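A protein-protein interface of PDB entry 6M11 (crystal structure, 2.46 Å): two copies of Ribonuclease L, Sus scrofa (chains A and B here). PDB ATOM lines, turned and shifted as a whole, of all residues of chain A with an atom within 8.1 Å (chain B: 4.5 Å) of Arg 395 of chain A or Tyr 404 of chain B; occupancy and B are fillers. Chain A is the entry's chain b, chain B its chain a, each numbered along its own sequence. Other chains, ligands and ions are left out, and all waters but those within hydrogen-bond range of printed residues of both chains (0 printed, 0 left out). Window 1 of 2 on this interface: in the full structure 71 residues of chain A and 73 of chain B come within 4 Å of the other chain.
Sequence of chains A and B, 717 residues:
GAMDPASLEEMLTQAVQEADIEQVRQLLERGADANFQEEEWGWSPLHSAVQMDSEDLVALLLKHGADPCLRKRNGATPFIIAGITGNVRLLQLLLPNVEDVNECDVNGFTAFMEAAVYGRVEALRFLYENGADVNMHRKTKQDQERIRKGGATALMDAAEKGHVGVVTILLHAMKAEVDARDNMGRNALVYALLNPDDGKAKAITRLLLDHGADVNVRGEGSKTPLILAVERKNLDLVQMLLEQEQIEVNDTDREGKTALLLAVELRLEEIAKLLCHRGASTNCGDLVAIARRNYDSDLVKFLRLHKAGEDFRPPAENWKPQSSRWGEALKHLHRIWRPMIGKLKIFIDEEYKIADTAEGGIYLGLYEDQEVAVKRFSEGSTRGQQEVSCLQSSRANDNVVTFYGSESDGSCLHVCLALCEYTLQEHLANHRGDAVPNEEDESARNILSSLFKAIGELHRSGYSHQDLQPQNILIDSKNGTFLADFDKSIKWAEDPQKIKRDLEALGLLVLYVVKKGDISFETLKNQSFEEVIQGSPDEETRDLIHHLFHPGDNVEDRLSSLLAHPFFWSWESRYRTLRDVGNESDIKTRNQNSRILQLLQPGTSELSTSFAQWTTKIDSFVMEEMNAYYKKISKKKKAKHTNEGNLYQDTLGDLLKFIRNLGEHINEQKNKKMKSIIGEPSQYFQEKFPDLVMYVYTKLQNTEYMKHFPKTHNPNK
Among the printed residues, merely in contact across the chains: Arg 395 of chain A with Arg 395 of chain B (3.8 Å), Arg 395 of chain A with Thr 402 of chain B (3.95 Å), Arg 395 of chain A with Phe 403 of chain B (3.7 Å) and Thr 402 of chain A with Arg 395 of chain B (3.8 Å).
Arg 395 of chain B touches its own counterpart, Arg 395 of chain A.
Arg 395 of chain A touches Tyr 404 of chain B, and with the chains exchanged Tyr 404 of chain A touches Arg 395 of chain B.
Of the 12 printed residues of chain B, 6 touch a printed residue of chain A.
Hydrophobic or aromatic side chains of chain B within 4 Å of the printed part of chain A: Tyr 404.
Printed residues of chain A that touch a printed residue of chain B: Glu 368, Gln 392, Arg 395, Thr 402 and Tyr 404.
Among the printed residues, 10 pairs touch across the chains.
Among the printed residues, Asp or Glu carboxylates within 4 Å of a Lys or Arg side-chain nitrogen of the other chain: Glu 368 of chain A with Arg 395 of chain B (3.1 Å) and Arg 395 of chain A with Glu 368 of chain B (3.8 Å).
The guanidinium group (NH2) of Arg 395 of chain B lies within hydrogen-bond range of the backbone carbonyl oxygen (O) of Phe 403 of chain B (2.8 Å).
The backbone NH (N) of Tyr 404 of chain B is in hydrogen-bond range of the backbone carbonyl oxygen (O) of Cys 416 of chain B.
The guanidinium group (NH1) of Arg 395 of chain B is in salt-bridge range of the side-chain carboxylate (OE1) of Glu 368 of chain A, at 3.1 Å.
The guanidinium group (NH1) of Arg 395 of chain A lies within salt-bridge range of the side-chain carboxylate (OE1) of Glu 368 of chain B, at 3.8 Å.
The backbone carbonyl oxygen (O) of Tyr 404 of chain B sits at hydrogen-bond distance from the guanidinium group (NH2) of Arg 395 of chain A (3.4 Å).
The side-chain amide nitrogen (NE2) of Gln 370 of chain B sits at hydrogen-bond distance from the backbone carbonyl oxygen (O) of Gln 392 of chain A, 3.1 Å away.
NH2 of Arg 395 of chain B sits at hydrogen-bond distance from O of Tyr 404 of chain A (3.3 Å).
The side-chain carboxylate (OE1) of Glu 368 of chain B lies within hydrogen-bond range of the side-chain amide nitrogen (NE2) of Gln 392 of chain A, 2.8 Å away.
Of chain A, only Arg 395 comes within 4 Å of Tyr 404 of chain B.
Printed residues of chain A within 4 Å of Thr 402 of chain B: Arg 395.
Of the printed residues of chain B, Thr 402 of chain A touches Arg 395 (3.8 Å).
Of the printed residues of chain A, Glu 368 of chain B touches Gln 392 and Arg 395.
The nearest printed residue of chain B that does not touch Arg 395 of chain A is Tyr 367 of chain B (4.7 Å).
The nearest residue of chain A that does not touch Tyr 404 of chain B is Tyr 404 of chain A (4.2 Å).
The nearest printed residue of chain A that does not touch Arg 395 of chain B is Phe 403 of chain A (4.1 Å).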
ATOM      1  N   LYS A 343      -6.434 -38.743  12.139  1.00  0.00           N
ATOM      2  CA  LYS A 343      -7.407 -37.654  12.150  1.00  0.00           C
ATOM      3  C   LYS A 343      -7.570 -36.958  10.790  1.00  0.00           C
ATOM      4  O   LYS A 343      -8.280 -35.941  10.682  1.00  0.00           O
ATOM      5  CB  LYS A 343      -7.016 -36.633  13.214  1.00  0.00           C
ATOM      6  CG  LYS A 343      -7.003 -37.122  14.680  1.00  0.00           C
ATOM      7  CD  LYS A 343      -6.335 -36.084  15.547  1.00  0.00           C
ATOM      8  CE  LYS A 343      -5.504 -36.657  16.685  1.00  0.00           C
ATOM      9  NZ  LYS A 343      -5.124 -35.573  17.620  1.00  0.00           N
ATOM     10  N   TYR A 367      -8.931 -32.291   8.500  1.00  0.00           N
ATOM     11  CA  TYR A 367      -8.238 -32.761   9.682  1.00  0.00           C
ATOM     12  C   TYR A 367      -9.095 -32.336  10.822  1.00  0.00           C
ATOM     13  O   TYR A 367      -9.325 -31.148  10.981  1.00  0.00           O
ATOM     14  CB  TYR A 367      -6.870 -32.079   9.753  1.00  0.00           C
ATOM     15  CG  TYR A 367      -6.036 -32.504  10.934  1.00  0.00           C
ATOM     16  CD1 TYR A 367      -5.239 -33.648  10.883  1.00  0.00           C
ATOM     17  CD2 TYR A 367      -6.100 -31.792  12.127  1.00  0.00           C
ATOM     18  CE1 TYR A 367      -4.496 -34.044  11.989  1.00  0.00           C
ATOM     19  CE2 TYR A 367      -5.366 -32.173  13.231  1.00  0.00           C
ATOM     20  CZ  TYR A 367      -4.564 -33.294  13.167  1.00  0.00           C
ATOM     21  OH  TYR A 367      -3.836 -33.634  14.294  1.00  0.00           O
ATOM     22  N   GLU A 368      -9.586 -33.307  11.594  1.00  0.00           N
ATOM     23  CA  GLU A 368     -10.660 -33.113  12.587  1.00  0.00           C
ATOM     24  C   GLU A 368     -11.761 -32.251  11.987  1.00  0.00           C
ATOM     25  O   GLU A 368     -12.237 -31.296  12.616  1.00  0.00           O
ATOM     26  CB  GLU A 368     -10.158 -32.444  13.870  1.00  0.00           C
ATOM     27  CG  GLU A 368      -8.774 -32.805  14.408  1.00  0.00           C
ATOM     28  CD  GLU A 368      -8.145 -31.651  15.221  1.00  0.00           C
ATOM     29  OE1 GLU A 368      -8.233 -30.471  14.771  1.00  0.00           O
ATOM     30  OE2 GLU A 368      -7.552 -31.906  16.310  1.00  0.00           O
ATOM     31  N   VAL A 388       8.678 -30.830  10.177  1.00  0.00           N
ATOM     32  CA  VAL A 388       7.840 -31.066  11.359  1.00  0.00           C
ATOM     33  C   VAL A 388       8.483 -30.408  12.565  1.00  0.00           C
ATOM     34  O   VAL A 388       7.821 -29.751  13.348  1.00  0.00           O
ATOM     35  CB  VAL A 388       7.441 -32.551  11.589  1.00  0.00           C
ATOM     36  CG1 VAL A 388       8.648 -33.470  11.692  1.00  0.00           C
ATOM     37  CG2 VAL A 388       6.567 -32.677  12.825  1.00  0.00           C
ATOM     38  N   SER A 389       9.796 -30.495  12.612  1.00  0.00           N
ATOM     39  CA  SER A 389      10.598 -29.983  13.708  1.00  0.00           C
ATOM     40  C   SER A 389      10.483 -28.471  13.806  1.00  0.00           C
ATOM     41  O   SER A 389      10.178 -27.937  14.864  1.00  0.00           O
ATOM     42  CB  SER A 389      12.061 -30.367  13.458  1.00  0.00           C
ATOM     43  OG  SER A 389      12.692 -30.847  14.622  1.00  0.00           O
ATOM     44  N   CYS A 390      10.728 -27.789  12.696  1.00  0.00           N
ATOM     45  CA  CYS A 390      10.621 -26.340  12.647  1.00  0.00           C
ATOM     46  C   CYS A 390       9.178 -25.850  12.816  1.00  0.00           C
ATOM     47  O   CYS A 390       8.975 -24.843  13.463  1.00  0.00           O
ATOM     48  CB  CYS A 390      11.318 -25.757  11.414  1.00  0.00           C
ATOM     49  SG  CYS A 390      11.067 -23.960  11.282  1.00  0.00           S
ATOM     50  N   LEU A 391       8.178 -26.544  12.271  1.00  0.00           N
ATOM     51  CA  LEU A 391       6.782 -26.177  12.547  1.00  0.00           C
ATOM     52  C   LEU A 391       6.398 -26.299  14.020  1.00  0.00           C
ATOM     53  O   LEU A 391       5.817 -25.380  14.571  1.00  0.00           O
ATOM     54  CB  LEU A 391       5.807 -26.926  11.656  1.00  0.00           C
ATOM     55  CG  LEU A 391       5.787 -26.515  10.177  1.00  0.00           C
ATOM     56  CD1 LEU A 391       5.256 -27.604   9.302  1.00  0.00           C
ATOM     57  CD2 LEU A 391       5.014 -25.224   9.981  1.00  0.00           C
ATOM     58  N   GLN A 392       6.768 -27.402  14.659  1.00  0.00           N
ATOM     59  CA  GLN A 392       6.676 -27.574  16.134  1.00  0.00           C
ATOM     60  C   GLN A 392       7.282 -26.481  17.008  1.00  0.00           C
ATOM     61  O   GLN A 392       6.772 -26.229  18.088  1.00  0.00           O
ATOM     62  CB  GLN A 392       7.228 -28.913  16.554  1.00  0.00           C
ATOM     63  CG  GLN A 392       6.244 -30.050  16.280  1.00  0.00           C
ATOM     64  CD  GLN A 392       6.922 -31.412  16.268  1.00  0.00           C
ATOM     65  OE1 GLN A 392       8.116 -31.530  16.534  1.00  0.00           O
ATOM     66  NE2 GLN A 392       6.163 -32.441  15.967  1.00  0.00           N
ATOM     67  N   SER A 393       8.320 -25.806  16.531  1.00  0.00           N
ATOM     68  CA  SER A 393       8.899 -24.681  17.273  1.00  0.00           C
ATOM     69  C   SER A 393       8.304 -23.324  16.902  1.00  0.00           C
ATOM     70  O   SER A 393       8.764 -22.284  17.424  1.00  0.00           O
ATOM     71  CB  SER A 393      10.432 -24.634  17.159  1.00  0.00           C
ATOM     72  OG  SER A 393      10.988 -25.892  16.908  1.00  0.00           O
ATOM     73  N   SER A 394       7.311 -23.318  16.014  1.00  0.00           N
ATOM     74  CA  SER A 394       6.832 -22.068  15.415  1.00  0.00           C
ATOM     75  C   SER A 394       5.374 -21.809  15.714  1.00  0.00           C
ATOM     76  O   SER A 394       4.826 -20.783  15.286  1.00  0.00           O
ATOM     77  CB  SER A 394       7.050 -22.086  13.890  1.00  0.00           C
ATOM     78  OG  SER A 394       8.420 -21.903  13.597  1.00  0.00           O
ATOM     79  N   ARG A 395       4.748 -22.696  16.477  1.00  0.00           N
ATOM     80  CA  ARG A 395       3.323 -22.575  16.790  1.00  0.00           C
ATOM     81  C   ARG A 395       2.902 -21.214  17.374  1.00  0.00           C
ATOM     82  O   ARG A 395       1.803 -20.764  17.109  1.00  0.00           O
ATOM     83  CB  ARG A 395       2.902 -23.746  17.664  1.00  0.00           C
ATOM     84  CG  ARG A 395       3.089 -25.051  16.934  1.00  0.00           C
ATOM     85  CD  ARG A 395       2.839 -26.260  17.809  1.00  0.00           C
ATOM     86  NE  ARG A 395       1.495 -26.760  17.543  1.00  0.00           N
ATOM     87  CZ  ARG A 395       1.207 -28.025  17.298  1.00  0.00           C
ATOM     88  NH1 ARG A 395       2.177 -28.949  17.342  1.00  0.00           N
ATOM     89  NH2 ARG A 395      -0.055 -28.358  17.032  1.00  0.00           N
ATOM     90  N   ALA A 396       3.800 -20.553  18.124  1.00  0.00           N
ATOM     91  CA  ALA A 396       3.606 -19.193  18.613  1.00  0.00           C
ATOM     92  C   ALA A 396       3.856 -18.106  17.564  1.00  0.00           C
ATOM     93  O   ALA A 396       3.470 -16.964  17.770  1.00  0.00           O
ATOM     94  CB  ALA A 396       4.500 -18.933  19.831  1.00  0.00           C
ATOM     95  N   ASN A 397       4.565 -18.422  16.480  1.00  0.00           N
ATOM     96  CA  ASN A 397       4.889 -17.413  15.466  1.00  0.00           C
ATOM     97  C   ASN A 397       3.682 -17.170  14.610  1.00  0.00           C
ATOM     98  O   ASN A 397       3.320 -18.018  13.801  1.00  0.00           O
ATOM     99  CB  ASN A 397       6.042 -17.910  14.619  1.00  0.00           C
ATOM    100  CG  ASN A 397       6.562 -16.887  13.641  1.00  0.00           C
ATOM    101  OD1 ASN A 397       5.873 -15.926  13.247  1.00  0.00           O
ATOM    102  ND2 ASN A 397       7.828 -17.097  13.238  1.00  0.00           N
ATOM    103  N   ASP A 398       3.053 -16.020  14.803  1.00  0.00           N
ATOM    104  CA  ASP A 398       1.766 -15.695  14.183  1.00  0.00           C
ATOM    105  C   ASP A 398       1.769 -15.519  12.697  1.00  0.00           C
ATOM    106  O   ASP A 398       0.696 -15.513  12.108  1.00  0.00           O
ATOM    107  CB  ASP A 398       1.217 -14.393  14.772  1.00  0.00           C
ATOM    108  CG  ASP A 398       0.698 -14.556  16.194  1.00  0.00           C
ATOM    109  OD1 ASP A 398       0.382 -15.707  16.602  1.00  0.00           O
ATOM    110  OD2 ASP A 398       0.596 -13.513  16.899  1.00  0.00           O
ATOM    111  N   ASN A 399       2.934 -15.321  12.084  1.00  0.00           N
ATOM    112  CA  ASN A 399       2.986 -15.157  10.637  1.00  0.00           C
ATOM    113  C   ASN A 399       3.680 -16.324  10.001  1.00  0.00           C
ATOM    114  O   ASN A 399       4.305 -16.197   8.969  1.00  0.00           O
ATOM    115  CB  ASN A 399       3.693 -13.869  10.337  1.00  0.00           C
ATOM    116  CG  ASN A 399       2.857 -12.677  10.706  1.00  0.00           C
ATOM    117  OD1 ASN A 399       3.188 -11.957  11.642  1.00  0.00           O
ATOM    118  ND2 ASN A 399       1.746 -12.463   9.966  1.00  0.00           N
ATOM    119  N   VAL A 400       3.566 -17.475  10.652  1.00  0.00           N
ATOM    120  CA  VAL A 400       3.932 -18.738  10.062  1.00  0.00           C
ATOM    121  C   VAL A 400       2.613 -19.496   9.907  1.00  0.00           C
ATOM    122  O   VAL A 400       1.653 -19.315  10.670  1.00  0.00           O
ATOM    123  CB  VAL A 400       4.983 -19.454  10.907  1.00  0.00           C
ATOM    124  CG1 VAL A 400       5.029 -20.939  10.628  1.00  0.00           C
ATOM    125  CG2 VAL A 400       6.347 -18.813  10.662  1.00  0.00           C
ATOM    126  N   VAL A 401       2.538 -20.253   8.841  1.00  0.00           N
ATOM    127  CA  VAL A 401       1.351 -20.966   8.488  1.00  0.00           C
ATOM    128  C   VAL A 401       1.003 -21.889   9.660  1.00  0.00           C
ATOM    129  O   VAL A 401       1.866 -22.559  10.183  1.00  0.00           O
ATOM    130  CB  VAL A 401       1.618 -21.682   7.122  1.00  0.00           C
ATOM    131  CG1 VAL A 401       2.764 -22.694   7.278  1.00  0.00           C
ATOM    132  CG2 VAL A 401       0.340 -22.315   6.612  1.00  0.00           C
ATOM    133  N   THR A 402      -0.252 -21.905  10.085  1.00  0.00           N
ATOM    134  CA  THR A 402      -0.650 -22.795  11.187  1.00  0.00           C
ATOM    135  C   THR A 402      -0.394 -24.275  10.914  1.00  0.00           C
ATOM    136  O   THR A 402      -0.791 -24.802   9.888  1.00  0.00           O
ATOM    137  CB  THR A 402      -2.115 -22.555  11.594  1.00  0.00           C
ATOM    138  OG1 THR A 402      -2.351 -21.144  11.689  1.00  0.00           O
ATOM    139  CG2 THR A 402      -2.441 -23.205  12.956  1.00  0.00           C
ATOM    140  N   PHE A 403       0.253 -24.931  11.852  1.00  0.00           N
ATOM    141  CA  PHE A 403       0.472 -26.370  11.877  1.00  0.00           C
ATOM    142  C   PHE A 403      -0.655 -27.090  12.645  1.00  0.00           C
ATOM    143  O   PHE A 403      -0.924 -26.754  13.790  1.00  0.00           O
ATOM    144  CB  PHE A 403       1.809 -26.604  12.588  1.00  0.00           C
ATOM    145  CG  PHE A 403       2.219 -28.041  12.677  1.00  0.00           C
ATOM    146  CD1 PHE A 403       2.165 -28.860  11.568  1.00  0.00           C
ATOM    147  CD2 PHE A 403       2.769 -28.544  13.841  1.00  0.00           C
ATOM    148  CE1 PHE A 403       2.580 -30.183  11.628  1.00  0.00           C
ATOM    149  CE2 PHE A 403       3.179 -29.870  13.936  1.00  0.00           C
ATOM    150  CZ  PHE A 403       3.058 -30.711  12.826  1.00  0.00           C
ATOM    151  N   TYR A 404      -1.370 -27.996  11.985  1.00  0.00           N
ATOM    152  CA  TYR A 404      -2.442 -28.713  12.645  1.00  0.00           C
ATOM    153  C   TYR A 404      -1.854 -29.961  13.302  1.00  0.00           C
ATOM    154  O   TYR A 404      -2.031 -30.182  14.509  1.00  0.00           O
ATOM    155  CB  TYR A 404      -3.606 -29.036  11.700  1.00  0.00           C
ATOM    156  CG  TYR A 404      -4.550 -27.884  11.428  1.00  0.00           C
ATOM    157  CD1 TYR A 404      -4.121 -26.698  10.799  1.00  0.00           C
ATOM    158  CD2 TYR A 404      -5.887 -27.974  11.779  1.00  0.00           C
ATOM    159  CE1 TYR A 404      -4.988 -25.636  10.591  1.00  0.00           C
ATOM    160  CE2 TYR A 404      -6.770 -26.915  11.521  1.00  0.00           C
ATOM    161  CZ  TYR A 404      -6.317 -25.766  10.937  1.00  0.00           C
ATOM    162  OH  TYR A 404      -7.187 -24.730  10.688  1.00  0.00           O
ATOM    163  N   GLY A 405      -1.118 -30.747  12.529  1.00  0.00           N
ATOM    164  CA  GLY A 405      -0.503 -31.963  13.041  1.00  0.00           C
ATOM    165  C   GLY A 405       0.046 -32.755  11.885  1.00  0.00           C
ATOM    166  O   GLY A 405      -0.194 -32.409  10.726  1.00  0.00           O
ATOM    167  N   SER A 406       0.770 -33.818  12.208  1.00  0.00           N
ATOM    168  CA  SER A 406       1.305 -34.761  11.246  1.00  0.00           C
ATOM    169  C   SER A 406       0.755 -36.150  11.517  1.00  0.00           C
ATOM    170  O   SER A 406       0.658 -36.564  12.663  1.00  0.00           O
ATOM    171  CB  SER A 406       2.839 -34.777  11.291  1.00  0.00           C
ATOM    172  OG  SER A 406       3.334 -35.217  12.543  1.00  0.00           O
ATOM    173  N   CYS A 416       0.026 -31.410   7.907  1.00  0.00           N
ATOM    174  CA  CYS A 416      -1.239 -30.675   7.684  1.00  0.00           C
ATOM    175  C   CYS A 416      -1.135 -29.231   8.139  1.00  0.00           C
ATOM    176  O   CYS A 416      -0.762 -28.953   9.266  1.00  0.00           O
ATOM    177  CB  CYS A 416      -2.414 -31.356   8.400  1.00  0.00           C
ATOM    178  SG  CYS A 416      -2.370 -33.170   8.275  1.00  0.00           S
ATOM    179  N   GLU A 457      10.911 -13.782  14.333  1.00  0.00           N
ATOM    180  CA  GLU A 457      10.511 -14.748  15.327  1.00  0.00           C
ATOM    181  C   GLU A 457      11.041 -16.138  15.009  1.00  0.00           C
ATOM    182  O   GLU A 457      11.336 -16.918  15.903  1.00  0.00           O
ATOM    183  CB  GLU A 457       9.005 -14.784  15.471  1.00  0.00           C
ATOM    184  CG  GLU A 457       8.619 -15.517  16.742  1.00  0.00           C
ATOM    185  CD  GLU A 457       7.290 -15.095  17.332  1.00  0.00           C
ATOM    186  OE1 GLU A 457       6.860 -13.915  17.175  1.00  0.00           O
ATOM    187  OE2 GLU A 457       6.682 -15.967  17.993  1.00  0.00           O
ATOM    188  N   SER A 461      13.438 -18.489  17.618  1.00  0.00           N
ATOM    189  CA  SER A 461      13.140 -19.895  17.910  1.00  0.00           C
ATOM    190  C   SER A 461      14.303 -20.831  17.551  1.00  0.00           C
ATOM    191  O   SER A 461      14.171 -22.061  17.674  1.00  0.00           O
ATOM    192  CB  SER A 461      11.914 -20.423  17.123  1.00  0.00           C
ATOM    193  OG  SER A 461      11.118 -19.434  16.523  1.00  0.00           O
ATOM    194  N   TYR B 367       4.385 -32.703  24.832  1.00  0.00           N
ATOM    195  CA  TYR B 367       3.625 -33.152  23.695  1.00  0.00           C
ATOM    196  C   TYR B 367       4.572 -33.022  22.551  1.00  0.00           C
ATOM    197  O   TYR B 367       4.997 -31.909  22.259  1.00  0.00           O
ATOM    198  CB  TYR B 367       2.414 -32.259  23.486  1.00  0.00           C
ATOM    199  CG  TYR B 367       1.525 -32.684  22.355  1.00  0.00           C
ATOM    200  CD1 TYR B 367       1.748 -32.221  21.064  1.00  0.00           C
ATOM    201  CD2 TYR B 367       0.421 -33.509  22.585  1.00  0.00           C
ATOM    202  CE1 TYR B 367       0.914 -32.606  20.010  1.00  0.00           C
ATOM    203  CE2 TYR B 367      -0.415 -33.895  21.548  1.00  0.00           C
ATOM    204  CZ  TYR B 367      -0.166 -33.441  20.259  1.00  0.00           C
ATOM    205  OH  TYR B 367      -0.987 -33.822  19.221  1.00  0.00           O
ATOM    206  N   GLU B 368       4.915 -34.156  21.932  1.00  0.00           N
ATOM    207  CA  GLU B 368       5.986 -34.237  20.929  1.00  0.00           C
ATOM    208  C   GLU B 368       7.210 -33.484  21.403  1.00  0.00           C
ATOM    209  O   GLU B 368       7.806 -32.702  20.657  1.00  0.00           O
ATOM    210  CB  GLU B 368       5.538 -33.701  19.573  1.00  0.00           C
ATOM    211  CG  GLU B 368       4.241 -34.299  19.061  1.00  0.00           C
ATOM    212  CD  GLU B 368       3.657 -33.558  17.856  1.00  0.00           C
ATOM    213  OE1 GLU B 368       3.895 -32.329  17.659  1.00  0.00           O
ATOM    214  OE2 GLU B 368       2.930 -34.231  17.098  1.00  0.00           O
ATOM    215  N   GLN B 370       7.461 -30.982  23.314  1.00  0.00           N
ATOM    216  CA  GLN B 370       7.210 -29.542  23.504  1.00  0.00           C
ATOM    217  C   GLN B 370       6.450 -29.413  24.819  1.00  0.00           C
ATOM    218  O   GLN B 370       5.531 -30.202  25.067  1.00  0.00           O
ATOM    219  CB  GLN B 370       6.347 -28.930  22.354  1.00  0.00           C
ATOM    220  CG  GLN B 370       6.672 -29.326  20.905  1.00  0.00           C
ATOM    221  CD  GLN B 370       8.028 -28.822  20.407  1.00  0.00           C
ATOM    222  OE1 GLN B 370       8.878 -29.623  19.957  1.00  0.00           O
ATOM    223  NE2 GLN B 370       8.241 -27.501  20.479  1.00  0.00           N
ATOM    224  N   VAL B 372       3.647 -28.189  27.402  1.00  0.00           N
ATOM    225  CA  VAL B 372       2.239 -27.846  27.289  1.00  0.00           C
ATOM    226  C   VAL B 372       1.526 -27.861  28.618  1.00  0.00           C
ATOM    227  O   VAL B 372       1.946 -28.505  29.555  1.00  0.00           O
ATOM    228  CB  VAL B 372       1.460 -28.826  26.365  1.00  0.00           C
ATOM    229  CG1 VAL B 372       1.801 -28.605  24.880  1.00  0.00           C
ATOM    230  CG2 VAL B 372       1.633 -30.281  26.802  1.00  0.00           C
ATOM    231  N   ARG B 395      -7.831 -22.190  15.718  1.00  0.00           N
ATOM    232  CA  ARG B 395      -6.467 -22.286  15.223  1.00  0.00           C
ATOM    233  C   ARG B 395      -5.942 -21.024  14.504  1.00  0.00           C
ATOM    234  O   ARG B 395      -4.790 -20.699  14.686  1.00  0.00           O
ATOM    235  CB  ARG B 395      -6.331 -23.579  14.399  1.00  0.00           C
ATOM    236  CG  ARG B 395      -6.898 -24.776  15.170  1.00  0.00           C
ATOM    237  CD  ARG B 395      -6.439 -26.149  14.763  1.00  0.00           C
ATOM    238  NE  ARG B 395      -5.204 -26.551  15.403  1.00  0.00           N
ATOM    239  CZ  ARG B 395      -4.958 -27.798  15.810  1.00  0.00           C
ATOM    240  NH1 ARG B 395      -5.883 -28.743  15.688  1.00  0.00           N
ATOM    241  NH2 ARG B 395      -3.797 -28.102  16.373  1.00  0.00           N
ATOM    242  N   THR B 402      -2.760 -21.375  21.854  1.00  0.00           N
ATOM    243  CA  THR B 402      -2.452 -22.388  20.867  1.00  0.00           C
ATOM    244  C   THR B 402      -2.836 -23.815  21.334  1.00  0.00           C
ATOM    245  O   THR B 402      -2.506 -24.248  22.439  1.00  0.00           O
ATOM    246  CB  THR B 402      -0.960 -22.357  20.496  1.00  0.00           C
ATOM    247  OG1 THR B 402      -0.527 -20.997  20.335  1.00  0.00           O
ATOM    248  CG2 THR B 402      -0.685 -23.168  19.214  1.00  0.00           C
ATOM    249  N   PHE B 403      -3.524 -24.524  20.460  1.00  0.00           N
ATOM    250  CA  PHE B 403      -3.977 -25.872  20.681  1.00  0.00           C
ATOM    251  C   PHE B 403      -3.041 -26.916  20.034  1.00  0.00           C
ATOM    252  O   PHE B 403      -2.984 -27.032  18.827  1.00  0.00           O
ATOM    253  CB  PHE B 403      -5.407 -25.987  20.114  1.00  0.00           C
ATOM    254  CG  PHE B 403      -6.014 -27.323  20.255  1.00  0.00           C
ATOM    255  CD1 PHE B 403      -5.907 -28.037  21.441  1.00  0.00           C
ATOM    256  CD2 PHE B 403      -6.734 -27.876  19.196  1.00  0.00           C
ATOM    257  CE1 PHE B 403      -6.526 -29.280  21.581  1.00  0.00           C
ATOM    258  CE2 PHE B 403      -7.361 -29.117  19.343  1.00  0.00           C
ATOM    259  CZ  PHE B 403      -7.259 -29.818  20.540  1.00  0.00           C
ATOM    260  N   TYR B 404      -2.443 -27.785  20.838  1.00  0.00           N
ATOM    261  CA  TYR B 404      -1.559 -28.803  20.321  1.00  0.00           C
ATOM    262  C   TYR B 404      -2.324 -30.003  19.811  1.00  0.00           C
ATOM    263  O   TYR B 404      -2.144 -30.406  18.683  1.00  0.00           O
ATOM    264  CB  TYR B 404      -0.446 -29.154  21.339  1.00  0.00           C
ATOM    265  CG  TYR B 404       0.707 -28.136  21.355  1.00  0.00           C
ATOM    266  CD1 TYR B 404       0.504 -26.820  21.801  1.00  0.00           C
ATOM    267  CD2 TYR B 404       1.971 -28.487  20.968  1.00  0.00           C
ATOM    268  CE1 TYR B 404       1.540 -25.891  21.840  1.00  0.00           C
ATOM    269  CE2 TYR B 404       3.020 -27.566  21.006  1.00  0.00           C
ATOM    270  CZ  TYR B 404       2.796 -26.268  21.429  1.00  0.00           C
ATOM    271  OH  TYR B 404       3.849 -25.376  21.449  1.00  0.00           O
ATOM    272  N   GLY B 405      -3.221 -30.521  20.621  1.00  0.00           N
ATOM    273  CA  GLY B 405      -4.114 -31.613  20.222  1.00  0.00           C
ATOM    274  C   GLY B 405      -4.649 -32.294  21.474  1.00  0.00           C
ATOM    275  O   GLY B 405      -4.277 -31.923  22.608  1.00  0.00           O
ATOM    276  N   CYS B 416      -4.319 -30.572  25.306  1.00  0.00           N
ATOM    277  CA  CYS B 416      -3.003 -29.961  25.394  1.00  0.00           C
ATOM    278  C   CYS B 416      -2.938 -28.569  24.761  1.00  0.00           C
ATOM    279  O   CYS B 416      -3.329 -28.376  23.613  1.00  0.00           O
ATOM    280  CB  CYS B 416      -1.968 -30.864  24.737  1.00  0.00           C
ATOM    281  SG  CYS B 416      -2.028 -32.535  25.399  1.00  0.00           S
ATOM    282  N   LEU B 417      -2.405 -27.625  25.528  1.00  0.00           N
ATOM    283  CA  LEU B 417      -2.410 -26.218  25.180  1.00  0.00           C
ATOM    284  C   LEU B 417      -1.030 -25.633  25.365  1.00  0.00           C
ATOM    285  O   LEU B 417      -0.235 -26.156  26.106  1.00  0.00           O
ATOM    286  CB  LEU B 417      -3.391 -25.455  26.068  1.00  0.00           C
ATOM    287  CG  LEU B 417      -4.827 -25.969  26.134  1.00  0.00           C
ATOM    288  CD1 LEU B 417      -5.556 -25.460  27.364  1.00  0.00           C
ATOM    289  CD2 LEU B 417      -5.519 -25.660  24.816  1.00  0.00           C
ATOM    290  N   ALA B 418      -0.747 -24.537  24.694  1.00  0.00           N
ATOM    291  CA  ALA B 418       0.525 -23.870  24.858  1.00  0.00           C
ATOM    292  C   ALA B 418       0.563 -23.456  26.316  1.00  0.00           C
ATOM    293  O   ALA B 418      -0.468 -23.167  26.919  1.00  0.00           O
ATOM    294  CB  ALA B 418       0.629 -22.646  23.936  1.00  0.00           C
